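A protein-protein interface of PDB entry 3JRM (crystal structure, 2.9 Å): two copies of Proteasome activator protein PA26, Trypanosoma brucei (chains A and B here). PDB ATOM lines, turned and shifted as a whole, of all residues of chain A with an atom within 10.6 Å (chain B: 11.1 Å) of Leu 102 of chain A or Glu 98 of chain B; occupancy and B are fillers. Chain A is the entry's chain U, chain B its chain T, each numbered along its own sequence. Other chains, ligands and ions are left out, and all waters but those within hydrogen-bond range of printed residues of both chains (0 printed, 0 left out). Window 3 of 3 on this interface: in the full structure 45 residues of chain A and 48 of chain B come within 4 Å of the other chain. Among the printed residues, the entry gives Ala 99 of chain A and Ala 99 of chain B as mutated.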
ATOM      1  N   PRO A  94     -24.810 -20.600  13.789  1.00  0.00           N
ATOM      2  CA  PRO A  94     -25.674 -19.442  13.904  1.00  0.00           C
ATOM      3  C   PRO A  94     -27.160 -19.719  13.663  1.00  0.00           C
ATOM      4  O   PRO A  94     -27.556 -20.829  13.296  1.00  0.00           O
ATOM      5  CB  PRO A  94     -25.117 -18.509  12.831  1.00  0.00           C
ATOM      6  CG  PRO A  94     -24.654 -19.432  11.767  1.00  0.00           C
ATOM      7  CD  PRO A  94     -24.131 -20.633  12.482  1.00  0.00           C
ATOM      8  N   GLU A  95     -27.954 -18.674  13.876  1.00  0.00           N
ATOM      9  CA  GLU A  95     -29.378 -18.668  13.587  1.00  0.00           C
ATOM     10  C   GLU A  95     -29.621 -19.369  12.264  1.00  0.00           C
ATOM     11  O   GLU A  95     -28.914 -19.081  11.283  1.00  0.00           O
ATOM     12  CB  GLU A  95     -29.842 -17.215  13.491  1.00  0.00           C
ATOM     13  CG  GLU A  95     -31.361 -16.991  13.329  1.00  0.00           C
ATOM     14  CD  GLU A  95     -31.704 -15.535  13.045  1.00  0.00           C
ATOM     15  OE1 GLU A  95     -30.777 -14.669  13.083  1.00  0.00           O
ATOM     16  OE2 GLU A  95     -32.884 -15.264  12.777  1.00  0.00           O
ATOM     17  N   LYS A  97     -31.135 -20.204   8.742  1.00  0.00           N
ATOM     18  CA  LYS A  97     -31.606 -19.351   7.646  1.00  0.00           C
ATOM     19  C   LYS A  97     -31.488 -20.132   6.342  1.00  0.00           C
ATOM     20  O   LYS A  97     -30.645 -20.997   6.246  1.00  0.00           O
ATOM     21  CB  LYS A  97     -30.736 -18.119   7.558  1.00  0.00           C
ATOM     22  CG  LYS A  97     -30.979 -17.083   8.616  1.00  0.00           C
ATOM     23  CD  LYS A  97     -30.005 -15.907   8.393  1.00  0.00           C
ATOM     24  CE  LYS A  97     -30.074 -14.865   9.506  1.00  0.00           C
ATOM     25  NZ  LYS A  97     -31.284 -14.021   9.327  1.00  0.00           N
ATOM     26  N   GLU A  98     -32.288 -19.822   5.325  1.00  0.00           N
ATOM     27  CA  GLU A  98     -32.162 -20.549   4.036  1.00  0.00           C
ATOM     28  C   GLU A  98     -31.003 -20.012   3.146  1.00  0.00           C
ATOM     29  O   GLU A  98     -30.749 -20.541   2.066  1.00  0.00           O
ATOM     30  CB  GLU A  98     -33.497 -20.559   3.246  1.00  0.00           C
ATOM     31  CG  GLU A  98     -34.693 -21.194   3.960  1.00  0.00           C
ATOM     32  CD  GLU A  98     -34.363 -22.516   4.667  1.00  0.00           C
ATOM     33  OE1 GLU A  98     -33.797 -23.408   3.992  1.00  0.00           O
ATOM     34  OE2 GLU A  98     -34.667 -22.666   5.896  1.00  0.00           O
ATOM     35  N   ALA A  99     -30.303 -18.974   3.592  1.00  0.00           N
ATOM     36  CA  ALA A  99     -29.213 -18.395   2.806  1.00  0.00           C
ATOM     37  C   ALA A  99     -28.146 -17.877   3.769  1.00  0.00           C
ATOM     38  O   ALA A  99     -28.312 -18.000   4.990  1.00  0.00           O
ATOM     39  CB  ALA A  99     -29.737 -17.279   1.889  1.00  0.00           C
ATOM     40  N   ASP A 100     -27.073 -17.305   3.220  1.00  0.00           N
ATOM     41  CA  ASP A 100     -25.895 -16.894   4.001  1.00  0.00           C
ATOM     42  C   ASP A 100     -25.326 -18.076   4.835  1.00  0.00           C
ATOM     43  O   ASP A 100     -25.021 -17.964   6.022  1.00  0.00           O
ATOM     44  CB  ASP A 100     -26.221 -15.681   4.885  1.00  0.00           C
ATOM     45  CG  ASP A 100     -24.966 -15.003   5.450  1.00  0.00           C
ATOM     46  OD1 ASP A 100     -23.839 -15.278   4.968  1.00  0.00           O
ATOM     47  OD2 ASP A 100     -25.113 -14.181   6.385  1.00  0.00           O
ATOM     48  N   ASN A 101     -25.180 -19.218   4.183  1.00  0.00           N
ATOM     49  CA  ASN A 101     -24.711 -20.420   4.834  1.00  0.00           C
ATOM     50  C   ASN A 101     -23.398 -20.942   4.272  1.00  0.00           C
ATOM     51  O   ASN A 101     -23.125 -22.119   4.365  1.00  0.00           O
ATOM     52  CB  ASN A 101     -25.764 -21.502   4.686  1.00  0.00           C
ATOM     53  CG  ASN A 101     -27.034 -21.181   5.408  1.00  0.00           C
ATOM     54  OD1 ASN A 101     -27.006 -20.793   6.582  1.00  0.00           O
ATOM     55  ND2 ASN A 101     -28.172 -21.373   4.722  1.00  0.00           N
ATOM     56  N   LEU A 102     -22.577 -20.072   3.695  1.00  0.00           N
ATOM     57  CA  LEU A 102     -21.250 -20.493   3.227  1.00  0.00           C
ATOM     58  C   LEU A 102     -20.338 -20.902   4.385  1.00  0.00           C
ATOM     59  O   LEU A 102     -19.631 -21.897   4.286  1.00  0.00           O
ATOM     60  CB  LEU A 102     -20.571 -19.392   2.421  1.00  0.00           C
ATOM     61  CG  LEU A 102     -21.273 -19.014   1.113  1.00  0.00           C
ATOM     62  CD1 LEU A 102     -20.380 -17.957   0.369  1.00  0.00           C
ATOM     63  CD2 LEU A 102     -21.635 -20.239   0.236  1.00  0.00           C
ATOM     64  N   GLY A 103     -20.370 -20.143   5.475  1.00  0.00           N
ATOM     65  CA  GLY A 103     -19.613 -20.463   6.680  1.00  0.00           C
ATOM     66  C   GLY A 103     -20.235 -21.624   7.425  1.00  0.00           C
ATOM     67  O   GLY A 103     -19.524 -22.502   7.883  1.00  0.00           O
ATOM     68  N   VAL A 104     -21.561 -21.633   7.537  1.00  0.00           N
ATOM     69  CA  VAL A 104     -22.253 -22.754   8.154  1.00  0.00           C
ATOM     70  C   VAL A 104     -21.809 -24.071   7.470  1.00  0.00           C
ATOM     71  O   VAL A 104     -21.557 -25.086   8.129  1.00  0.00           O
ATOM     72  CB  VAL A 104     -23.793 -22.573   8.084  1.00  0.00           C
ATOM     73  CG1 VAL A 104     -24.486 -23.822   8.610  1.00  0.00           C
ATOM     74  CG2 VAL A 104     -24.208 -21.318   8.845  1.00  0.00           C
ATOM     75  N   ALA A 105     -21.688 -24.052   6.146  1.00  0.00           N
ATOM     76  CA  ALA A 105     -21.304 -25.260   5.420  1.00  0.00           C
ATOM     77  C   ALA A 105     -19.907 -25.722   5.861  1.00  0.00           C
ATOM     78  O   ALA A 105     -19.686 -26.916   5.986  1.00  0.00           O
ATOM     79  CB  ALA A 105     -21.347 -25.031   3.911  1.00  0.00           C
ATOM     80  N   VAL A 106     -18.989 -24.770   6.096  1.00  0.00           N
ATOM     81  CA  VAL A 106     -17.654 -25.077   6.612  1.00  0.00           C
ATOM     82  C   VAL A 106     -17.753 -25.705   7.996  1.00  0.00           C
ATOM     83  O   VAL A 106     -17.062 -26.672   8.287  1.00  0.00           O
ATOM     84  CB  VAL A 106     -16.738 -23.827   6.697  1.00  0.00           C
ATOM     85  CG1 VAL A 106     -15.437 -24.156   7.437  1.00  0.00           C
ATOM     86  CG2 VAL A 106     -16.418 -23.301   5.300  1.00  0.00           C
ATOM     87  N   GLN A 107     -18.610 -25.145   8.846  1.00  0.00           N
ATOM     88  CA  GLN A 107     -18.845 -25.702  10.171  1.00  0.00           C
ATOM     89  C   GLN A 107     -19.322 -27.164  10.077  1.00  0.00           C
ATOM     90  O   GLN A 107     -18.694 -28.046  10.662  1.00  0.00           O
ATOM     91  CB  GLN A 107     -19.828 -24.845  10.977  1.00  0.00           C
ATOM     92  CG  GLN A 107     -19.292 -23.453  11.354  1.00  0.00           C
ATOM     93  CD  GLN A 107     -20.294 -22.628  12.168  1.00  0.00           C
ATOM     94  OE1 GLN A 107     -21.497 -22.639  11.894  1.00  0.00           O
ATOM     95  NE2 GLN A 107     -19.795 -21.904  13.162  1.00  0.00           N
ATOM     96  N   HIS A 108     -20.396 -27.435   9.331  1.00  0.00           N
ATOM     97  CA  HIS A 108     -20.890 -28.822   9.202  1.00  0.00           C
ATOM     98  C   HIS A 108     -19.839 -29.736   8.557  1.00  0.00           C
ATOM     99  O   HIS A 108     -19.712 -30.888   8.945  1.00  0.00           O
ATOM    100  CB  HIS A 108     -22.257 -28.908   8.487  1.00  0.00           C
ATOM    101  CG  HIS A 108     -23.388 -28.273   9.261  1.00  0.00           C
ATOM    102  ND1 HIS A 108     -23.616 -28.515  10.605  1.00  0.00           N
ATOM    103  CD2 HIS A 108     -24.353 -27.393   8.876  1.00  0.00           C
ATOM    104  CE1 HIS A 108     -24.660 -27.809  11.016  1.00  0.00           C
ATOM    105  NE2 HIS A 108     -25.121 -27.117   9.987  1.00  0.00           N
ATOM    106  N   ALA A 109     -19.060 -29.207   7.626  1.00  0.00           N
ATOM    107  CA  ALA A 109     -18.029 -29.992   6.963  1.00  0.00           C
ATOM    108  C   ALA A 109     -16.993 -30.506   7.958  1.00  0.00           C
ATOM    109  O   ALA A 109     -16.661 -31.693   7.956  1.00  0.00           O
ATOM    110  CB  ALA A 109     -17.366 -29.185   5.848  1.00  0.00           C
ATOM    111  N   VAL A 110     -16.494 -29.616   8.814  1.00  0.00           N
ATOM    112  CA  VAL A 110     -15.470 -29.973   9.797  1.00  0.00           C
ATOM    113  C   VAL A 110     -16.047 -30.799  10.958  1.00  0.00           C
ATOM    114  O   VAL A 110     -15.386 -31.708  11.483  1.00  0.00           O
ATOM    115  CB  VAL A 110     -14.753 -28.738  10.336  1.00  0.00           C
ATOM    116  CG1 VAL A 110     -13.735 -29.107  11.378  1.00  0.00           C
ATOM    117  CG2 VAL A 110     -14.070 -28.046   9.205  1.00  0.00           C
ATOM    118  N   ASN A 212      -9.484 -23.679   8.099  1.00  0.00           N
ATOM    119  CA  ASN A 212     -10.885 -23.251   8.128  1.00  0.00           C
ATOM    120  C   ASN A 212     -11.323 -22.510   9.385  1.00  0.00           C
ATOM    121  O   ASN A 212     -12.477 -22.123   9.499  1.00  0.00           O
ATOM    122  CB  ASN A 212     -11.803 -24.463   7.946  1.00  0.00           C
ATOM    123  CG  ASN A 212     -11.757 -25.027   6.543  1.00  0.00           C
ATOM    124  OD1 ASN A 212     -12.234 -24.396   5.601  1.00  0.00           O
ATOM    125  ND2 ASN A 212     -11.211 -26.228   6.400  1.00  0.00           N
ATOM    126  N   LYS A 214     -11.201 -19.649  10.827  1.00  0.00           N
ATOM    127  CA  LYS A 214     -11.809 -18.313  10.869  1.00  0.00           C
ATOM    128  C   LYS A 214     -13.294 -18.396  10.655  1.00  0.00           C
ATOM    129  O   LYS A 214     -14.047 -17.769  11.387  1.00  0.00           O
ATOM    130  CB  LYS A 214     -11.194 -17.377   9.845  1.00  0.00           C
ATOM    131  CG  LYS A 214      -9.909 -16.735  10.324  1.00  0.00           C
ATOM    132  CD  LYS A 214      -9.253 -15.954   9.200  1.00  0.00           C
ATOM    133  CE  LYS A 214      -7.870 -15.475   9.580  1.00  0.00           C
ATOM    134  NZ  LYS A 214      -7.431 -14.416   8.635  1.00  0.00           N
ATOM    135  N   LYS A 215     -13.719 -19.201   9.685  1.00  0.00           N
ATOM    136  CA  LYS A 215     -15.152 -19.418   9.457  1.00  0.00           C
ATOM    137  C   LYS A 215     -15.785 -20.294  10.498  1.00  0.00           C
ATOM    138  O   LYS A 215     -16.975 -20.178  10.745  1.00  0.00           O
ATOM    139  CB  LYS A 215     -15.405 -20.060   8.106  1.00  0.00           C
ATOM    140  CG  LYS A 215     -14.956 -19.252   6.937  1.00  0.00           C
ATOM    141  CD  LYS A 215     -15.901 -18.143   6.639  1.00  0.00           C
ATOM    142  CE  LYS A 215     -15.500 -17.446   5.380  1.00  0.00           C
ATOM    143  NZ  LYS A 215     -16.294 -16.200   5.279  1.00  0.00           N
ATOM    144  N   LEU A 216     -15.016 -21.203  11.093  1.00  0.00           N
ATOM    145  CA  LEU A 216     -15.549 -22.021  12.206  1.00  0.00           C
ATOM    146  C   LEU A 216     -16.037 -21.137  13.367  1.00  0.00           C
ATOM    147  O   LEU A 216     -17.133 -21.360  13.871  1.00  0.00           O
ATOM    148  CB  LEU A 216     -14.544 -23.066  12.675  1.00  0.00           C
ATOM    149  CG  LEU A 216     -14.196 -24.139  11.644  1.00  0.00           C
ATOM    150  CD1 LEU A 216     -13.130 -25.058  12.210  1.00  0.00           C
ATOM    151  CD2 LEU A 216     -15.405 -24.941  11.210  1.00  0.00           C
ATOM    152  N   ILE A 217     -15.259 -20.096  13.709  1.00  0.00           N
ATOM    153  CA  ILE A 217     -15.627 -19.142  14.769  1.00  0.00           C
ATOM    154  C   ILE A 217     -16.626 -18.056  14.290  1.00  0.00           C
ATOM    155  O   ILE A 217     -17.627 -17.818  14.961  1.00  0.00           O
ATOM    156  CB  ILE A 217     -14.386 -18.447  15.385  1.00  0.00           C
ATOM    157  CG1 ILE A 217     -13.312 -19.465  15.776  1.00  0.00           C
ATOM    158  CG2 ILE A 217     -14.795 -17.592  16.572  1.00  0.00           C
ATOM    159  CD1 ILE A 217     -13.775 -20.560  16.663  1.00  0.00           C
ATOM    160  N   GLN A 218     -16.346 -17.400  13.157  1.00  0.00           N
ATOM    161  CA  GLN A 218     -17.237 -16.363  12.574  1.00  0.00           C
ATOM    162  C   GLN A 218     -17.723 -16.790  11.185  1.00  0.00           C
ATOM    163  O   GLN A 218     -17.136 -16.409  10.172  1.00  0.00           O
ATOM    164  CB  GLN A 218     -16.538 -15.000  12.453  1.00  0.00           C
ATOM    165  CG  GLN A 218     -16.065 -14.329  13.762  1.00  0.00           C
ATOM    166  CD  GLN A 218     -17.180 -14.098  14.821  1.00  0.00           C
ATOM    167  OE1 GLN A 218     -18.386 -14.036  14.506  1.00  0.00           O
ATOM    168  NE2 GLN A 218     -16.761 -13.963  16.087  1.00  0.00           N
ATOM    169  N   PRO A 219     -18.794 -17.599  11.136  1.00  0.00           N
ATOM    170  CA  PRO A 219     -19.325 -18.133   9.880  1.00  0.00           C
ATOM    171  C   PRO A 219     -20.106 -17.158   9.031  1.00  0.00           C
ATOM    172  O   PRO A 219     -20.565 -17.541   7.973  1.00  0.00           O
ATOM    173  CB  PRO A 219     -20.261 -19.255  10.354  1.00  0.00           C
ATOM    174  CG  PRO A 219     -20.660 -18.876  11.707  1.00  0.00           C
ATOM    175  CD  PRO A 219     -19.465 -18.197  12.304  1.00  0.00           C
ATOM    176  N   ARG A 220     -20.301 -15.938   9.516  1.00  0.00           N
ATOM    177  CA  ARG A 220     -21.022 -14.874   8.809  1.00  0.00           C
ATOM    178  C   ARG A 220     -20.377 -13.540   9.153  1.00  0.00           C
ATOM    179  O   ARG A 220     -19.932 -13.337  10.287  1.00  0.00           O
ATOM    180  CB  ARG A 220     -22.483 -14.826   9.262  1.00  0.00           C
ATOM    181  CG  ARG A 220     -23.353 -15.936   8.725  1.00  0.00           C
ATOM    182  CD  ARG A 220     -24.776 -15.889   9.260  1.00  0.00           C
ATOM    183  NE  ARG A 220     -25.521 -17.027   8.729  1.00  0.00           N
ATOM    184  CZ  ARG A 220     -26.614 -17.575   9.263  1.00  0.00           C
ATOM    185  NH1 ARG A 220     -27.169 -17.116  10.363  1.00  0.00           N
ATOM    186  NH2 ARG A 220     -27.166 -18.603   8.669  1.00  0.00           N
ATOM    187  N   THR A 221     -20.298 -12.646   8.170  1.00  0.00           N
ATOM    188  CA  THR A 221     -20.001 -11.208   8.419  1.00  0.00           C
ATOM    189  C   THR A 221     -20.734 -10.473   7.328  1.00  0.00           C
ATOM    190  O   THR A 221     -20.522 -10.767   6.157  1.00  0.00           O
ATOM    191  CB  THR A 221     -18.495 -10.876   8.344  1.00  0.00           C
ATOM    192  OG1 THR A 221     -17.921 -11.653   7.289  1.00  0.00           O
ATOM    193  CG2 THR A 221     -17.744 -11.184   9.714  1.00  0.00           C
ATOM    194  N   PRO B  94      -7.732 -28.395   0.563  1.00  0.00           N
ATOM    195  CA  PRO B  94      -7.714 -26.982   0.851  1.00  0.00           C
ATOM    196  C   PRO B  94      -8.929 -26.459   1.603  1.00  0.00           C
ATOM    197  O   PRO B  94      -9.908 -27.178   1.807  1.00  0.00           O
ATOM    198  CB  PRO B  94      -7.661 -26.367  -0.539  1.00  0.00           C
ATOM    199  CG  PRO B  94      -8.444 -27.278  -1.361  1.00  0.00           C
ATOM    200  CD  PRO B  94      -8.183 -28.649  -0.815  1.00  0.00           C
ATOM    201  N   GLU B  95      -8.849 -25.187   1.974  1.00  0.00           N
ATOM    202  CA  GLU B  95      -9.955 -24.453   2.589  1.00  0.00           C
ATOM    203  C   GLU B  95     -11.297 -24.775   1.915  1.00  0.00           C
ATOM    204  O   GLU B  95     -11.383 -24.721   0.690  1.00  0.00           O
ATOM    205  CB  GLU B  95      -9.668 -22.961   2.426  1.00  0.00           C
ATOM    206  CG  GLU B  95     -10.610 -21.990   3.141  1.00  0.00           C
ATOM    207  CD  GLU B  95     -10.311 -20.533   2.772  1.00  0.00           C
ATOM    208  OE1 GLU B  95      -9.345 -20.258   2.015  1.00  0.00           O
ATOM    209  OE2 GLU B  95     -11.048 -19.645   3.230  1.00  0.00           O
ATOM    210  N   HIS B  96     -12.328 -25.071   2.696  1.00  0.00           N
ATOM    211  CA  HIS B  96     -13.634 -25.438   2.150  1.00  0.00           C
ATOM    212  C   HIS B  96     -14.303 -24.249   1.522  1.00  0.00           C
ATOM    213  O   HIS B  96     -14.388 -23.211   2.134  1.00  0.00           O
ATOM    214  CB  HIS B  96     -14.541 -25.983   3.260  1.00  0.00           C
ATOM    215  CG  HIS B  96     -15.842 -26.545   2.774  1.00  0.00           C
ATOM    216  ND1 HIS B  96     -16.055 -27.899   2.606  1.00  0.00           N
ATOM    217  CD2 HIS B  96     -17.008 -25.936   2.440  1.00  0.00           C
ATOM    218  CE1 HIS B  96     -17.288 -28.096   2.172  1.00  0.00           C
ATOM    219  NE2 HIS B  96     -17.890 -26.921   2.069  1.00  0.00           N
ATOM    220  N   LYS B  97     -14.809 -24.433   0.308  1.00  0.00           N
ATOM    221  CA  LYS B  97     -15.434 -23.376  -0.500  1.00  0.00           C
ATOM    222  C   LYS B  97     -16.512 -23.995  -1.404  1.00  0.00           C
ATOM    223  O   LYS B  97     -16.395 -25.158  -1.767  1.00  0.00           O
ATOM    224  CB  LYS B  97     -14.390 -22.743  -1.393  1.00  0.00           C
ATOM    225  CG  LYS B  97     -13.420 -21.832  -0.706  1.00  0.00           C
ATOM    226  CD  LYS B  97     -12.428 -21.284  -1.757  1.00  0.00           C
ATOM    227  CE  LYS B  97     -11.318 -20.460  -1.143  1.00  0.00           C
ATOM    228  NZ  LYS B  97     -11.816 -19.120  -0.732  1.00  0.00           N
ATOM    229  N   GLU B  98     -17.534 -23.230  -1.793  1.00  0.00           N
ATOM    230  CA  GLU B  98     -18.596 -23.772  -2.658  1.00  0.00           C
ATOM    231  C   GLU B  98     -18.206 -23.800  -4.145  1.00  0.00           C
ATOM    232  O   GLU B  98     -18.971 -24.305  -4.957  1.00  0.00           O
ATOM    233  CB  GLU B  98     -19.946 -23.052  -2.458  1.00  0.00           C
ATOM    234  CG  GLU B  98     -20.535 -23.076  -1.047  1.00  0.00           C
ATOM    235  CD  GLU B  98     -20.432 -24.433  -0.332  1.00  0.00           C
ATOM    236  OE1 GLU B  98     -20.951 -25.408  -0.866  1.00  0.00           O
ATOM    237  OE2 GLU B  98     -19.847 -24.547   0.777  1.00  0.00           O
ATOM    238  N   ALA B  99     -17.020 -23.306  -4.489  1.00  0.00           N
ATOM    239  CA  ALA B  99     -16.540 -23.270  -5.870  1.00  0.00           C
ATOM    240  C   ALA B  99     -15.033 -23.460  -5.886  1.00  0.00           C
ATOM    241  O   ALA B  99     -14.410 -23.592  -4.824  1.00  0.00           O
ATOM    242  CB  ALA B  99     -16.898 -21.960  -6.513  1.00  0.00           C
ATOM    243  N   ASP B 100     -14.451 -23.462  -7.088  1.00  0.00           N
ATOM    244  CA  ASP B 100     -13.017 -23.773  -7.290  1.00  0.00           C
ATOM    245  C   ASP B 100     -12.638 -25.140  -6.683  1.00  0.00           C
ATOM    246  O   ASP B 100     -11.641 -25.285  -5.983  1.00  0.00           O
ATOM    247  CB  ASP B 100     -12.144 -22.649  -6.725  1.00  0.00           C
ATOM    248  CG  ASP B 100     -10.707 -22.726  -7.180  1.00  0.00           C
ATOM    249  OD1 ASP B 100     -10.393 -23.529  -8.066  1.00  0.00           O
ATOM    250  OD2 ASP B 100      -9.877 -21.972  -6.637  1.00  0.00           O
ATOM    251  N   ASN B 101     -13.460 -26.141  -6.968  1.00  0.00           N
ATOM    252  CA  ASN B 101     -13.284 -27.460  -6.424  1.00  0.00           C
ATOM    253  C   ASN B 101     -13.030 -28.505  -7.493  1.00  0.00           C
ATOM    254  O   ASN B 101     -13.315 -29.657  -7.271  1.00  0.00           O
ATOM    255  CB  ASN B 101     -14.520 -27.849  -5.649  1.00  0.00           C
ATOM    256  CG  ASN B 101     -14.733 -27.002  -4.460  1.00  0.00           C
ATOM    257  OD1 ASN B 101     -13.817 -26.766  -3.692  1.00  0.00           O
ATOM    258  ND2 ASN B 101     -15.959 -26.570  -4.264  1.00  0.00           N
ATOM    259  N   LEU B 102     -12.477 -28.118  -8.641  1.00  0.00           N
ATOM    260  CA  LEU B 102     -12.124 -29.096  -9.668  1.00  0.00           C
ATOM    261  C   LEU B 102     -11.015 -30.002  -9.200  1.00  0.00           C
ATOM    262  O   LEU B 102     -11.068 -31.194  -9.459  1.00  0.00           O
ATOM    263  CB  LEU B 102     -11.717 -28.416 -10.973  1.00  0.00           C
ATOM    264  CG  LEU B 102     -12.807 -27.597 -11.669  1.00  0.00           C
ATOM    265  CD1 LEU B 102     -12.209 -27.092 -12.994  1.00  0.00           C
ATOM    266  CD2 LEU B 102     -14.146 -28.352 -11.837  1.00  0.00           C
ATOM    267  N   GLY B 103     -10.023 -29.446  -8.514  1.00  0.00           N
ATOM    268  CA  GLY B 103      -8.920 -30.230  -7.959  1.00  0.00           C
ATOM    269  C   GLY B 103      -9.336 -31.009  -6.737  1.00  0.00           C
ATOM    270  O   GLY B 103      -8.968 -32.153  -6.584  1.00  0.00           O
ATOM    271  N   VAL B 104     -10.119 -30.382  -5.872  1.00  0.00           N
ATOM    272  CA  VAL B 104     -10.649 -31.054  -4.699  1.00  0.00           C
ATOM    273  C   VAL B 104     -11.405 -32.322  -5.134  1.00  0.00           C
ATOM    274  O   VAL B 104     -11.319 -33.363  -4.487  1.00  0.00           O
ATOM    275  CB  VAL B 104     -11.552 -30.099  -3.884  1.00  0.00           C
ATOM    276  CG1 VAL B 104     -12.191 -30.795  -2.698  1.00  0.00           C
ATOM    277  CG2 VAL B 104     -10.741 -28.903  -3.426  1.00  0.00           C
ATOM    278  N   ALA B 105     -12.126 -32.249  -6.252  1.00  0.00           N
ATOM    279  CA  ALA B 105     -12.870 -33.418  -6.750  1.00  0.00           C
ATOM    280  C   ALA B 105     -11.913 -34.561  -7.138  1.00  0.00           C
ATOM    281  O   ALA B 105     -12.221 -35.720  -6.880  1.00  0.00           O
ATOM    282  CB  ALA B 105     -13.770 -33.048  -7.913  1.00  0.00           C
ATOM    283  N   ARG B 220      -5.562 -26.279  -6.576  1.00  0.00           N
ATOM    284  CA  ARG B 220      -5.993 -24.929  -6.951  1.00  0.00           C
ATOM    285  C   ARG B 220      -4.788 -24.135  -7.409  1.00  0.00           C
ATOM    286  O   ARG B 220      -3.722 -24.266  -6.819  1.00  0.00           O
ATOM    287  CB  ARG B 220      -6.609 -24.201  -5.753  1.00  0.00           C
ATOM    288  CG  ARG B 220      -7.981 -24.651  -5.387  1.00  0.00           C
ATOM    289  CD  ARG B 220      -8.521 -23.969  -4.170  1.00  0.00           C
ATOM    290  NE  ARG B 220      -9.834 -24.521  -3.855  1.00  0.00           N
ATOM    291  CZ  ARG B 220     -10.437 -24.486  -2.668  1.00  0.00           C
ATOM    292  NH1 ARG B 220      -9.895 -23.908  -1.605  1.00  0.00           N
ATOM    293  NH2 ARG B 220     -11.627 -25.033  -2.542  1.00  0.00           N
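Leu 102 of chain A touches just one residue of chain B: Glu 98 (3.3 Å).
Glu 98 of chain B touches two residues of chain A.
No residue of chain B comes within 4 Å of Asp 100 of chain A.
No residue of chain B comes within 4 Å of Asn 101 of chain A.
No residue of chain B comes within 4 Å of Val 104 of chain A.
Ala 105 of chain A touches just one residue of chain B: Glu 98.
Val 106 of chain A touches one residue of chain B.
No residue of chain A comes within 4 Å of Ala 99 of chain B.
Of the printed residues of chain A, Glu 95 of chain B touches Asn 212.
Of the printed residues of chain B, Asn 212 of chain A touches Glu 95 and His 96.
Printed residues of chain A within 4 Å of His 96 of chain B: Val 106, Ala 109 and Asn 212.
The nearest residue of chain B that does not touch Leu 102 of chain A is His 96 of chain B (5.2 Å).
Leu 102 of chain A touches Glu 98 of chain B, but with the chains exchanged Glu 98 of chain A does not touch Leu 102 of chain B (22.5 Å).
Ala 105 of chain A touches Glu 98 of chain B, but with the chains exchanged Glu 98 of chain A does not touch Ala 105 of chain B (23.3 Å).
Of the 6 pairs that touch across the chains among the printed residues, none has its exchanged pair printed and touching as well.
OE2 of Glu 98 of chain B sits at hydrogen-bond distance from NE2 of His 96 of chain B, at 3.3 Å.
The backbone carbonyl oxygen of Glu 95 of chain B sits at hydrogen-bond distance from the guanidinium group of Arg 220 of chain B (2.9 Å).
The side-chain amino group (NZ) of Lys 97 of chain B lies within salt-bridge range of the side-chain carboxylate (OE1) of Glu 95 of chain B.
Among the printed residues, merely in contact across the chains: Leu 102 of chain A with Glu 98 of chain B (3.3 Å), Ala 105 of chain A with Glu 98 of chain B (3.5 Å), Val 106 of chain A with His 96 of chain B (3.8 Å), Ala 109 of chain A with His 96 of chain B (3.7 Å) and Asn 212 of chain A with Glu 95 of chain B (3.8 Å).
Of the 25 printed residues of chain A, 5 touch a printed residue of chain B.
Printed residues of chain A that touch a printed residue of chain B: Leu 102, Ala 105, Val 106, Ala 109 and Asn 212.
Hydrophobic or aromatic side chains of chain A that line the printed part of chain B: Leu 102, Ala 105, Val 106 and Ala 109.
Of the 13 printed residues of chain B, 3 touch a printed residue of chain A.
Hydrophobic or aromatic side chains of chain B within 4 Å of the printed part of chain A: His 96.
Among the printed residues, 6 pairs touch across the chains.
Among the printed residues, no Asp or Glu carboxylate lies within 4 Å of a Lys or Arg side-chain nitrogen of the other chain.
The side-chain amide oxygen (OD1) of Asn 212 of chain A sits at hydrogen-bond distance from the backbone NH (N) of His 96 of chain B (3.0 Å).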
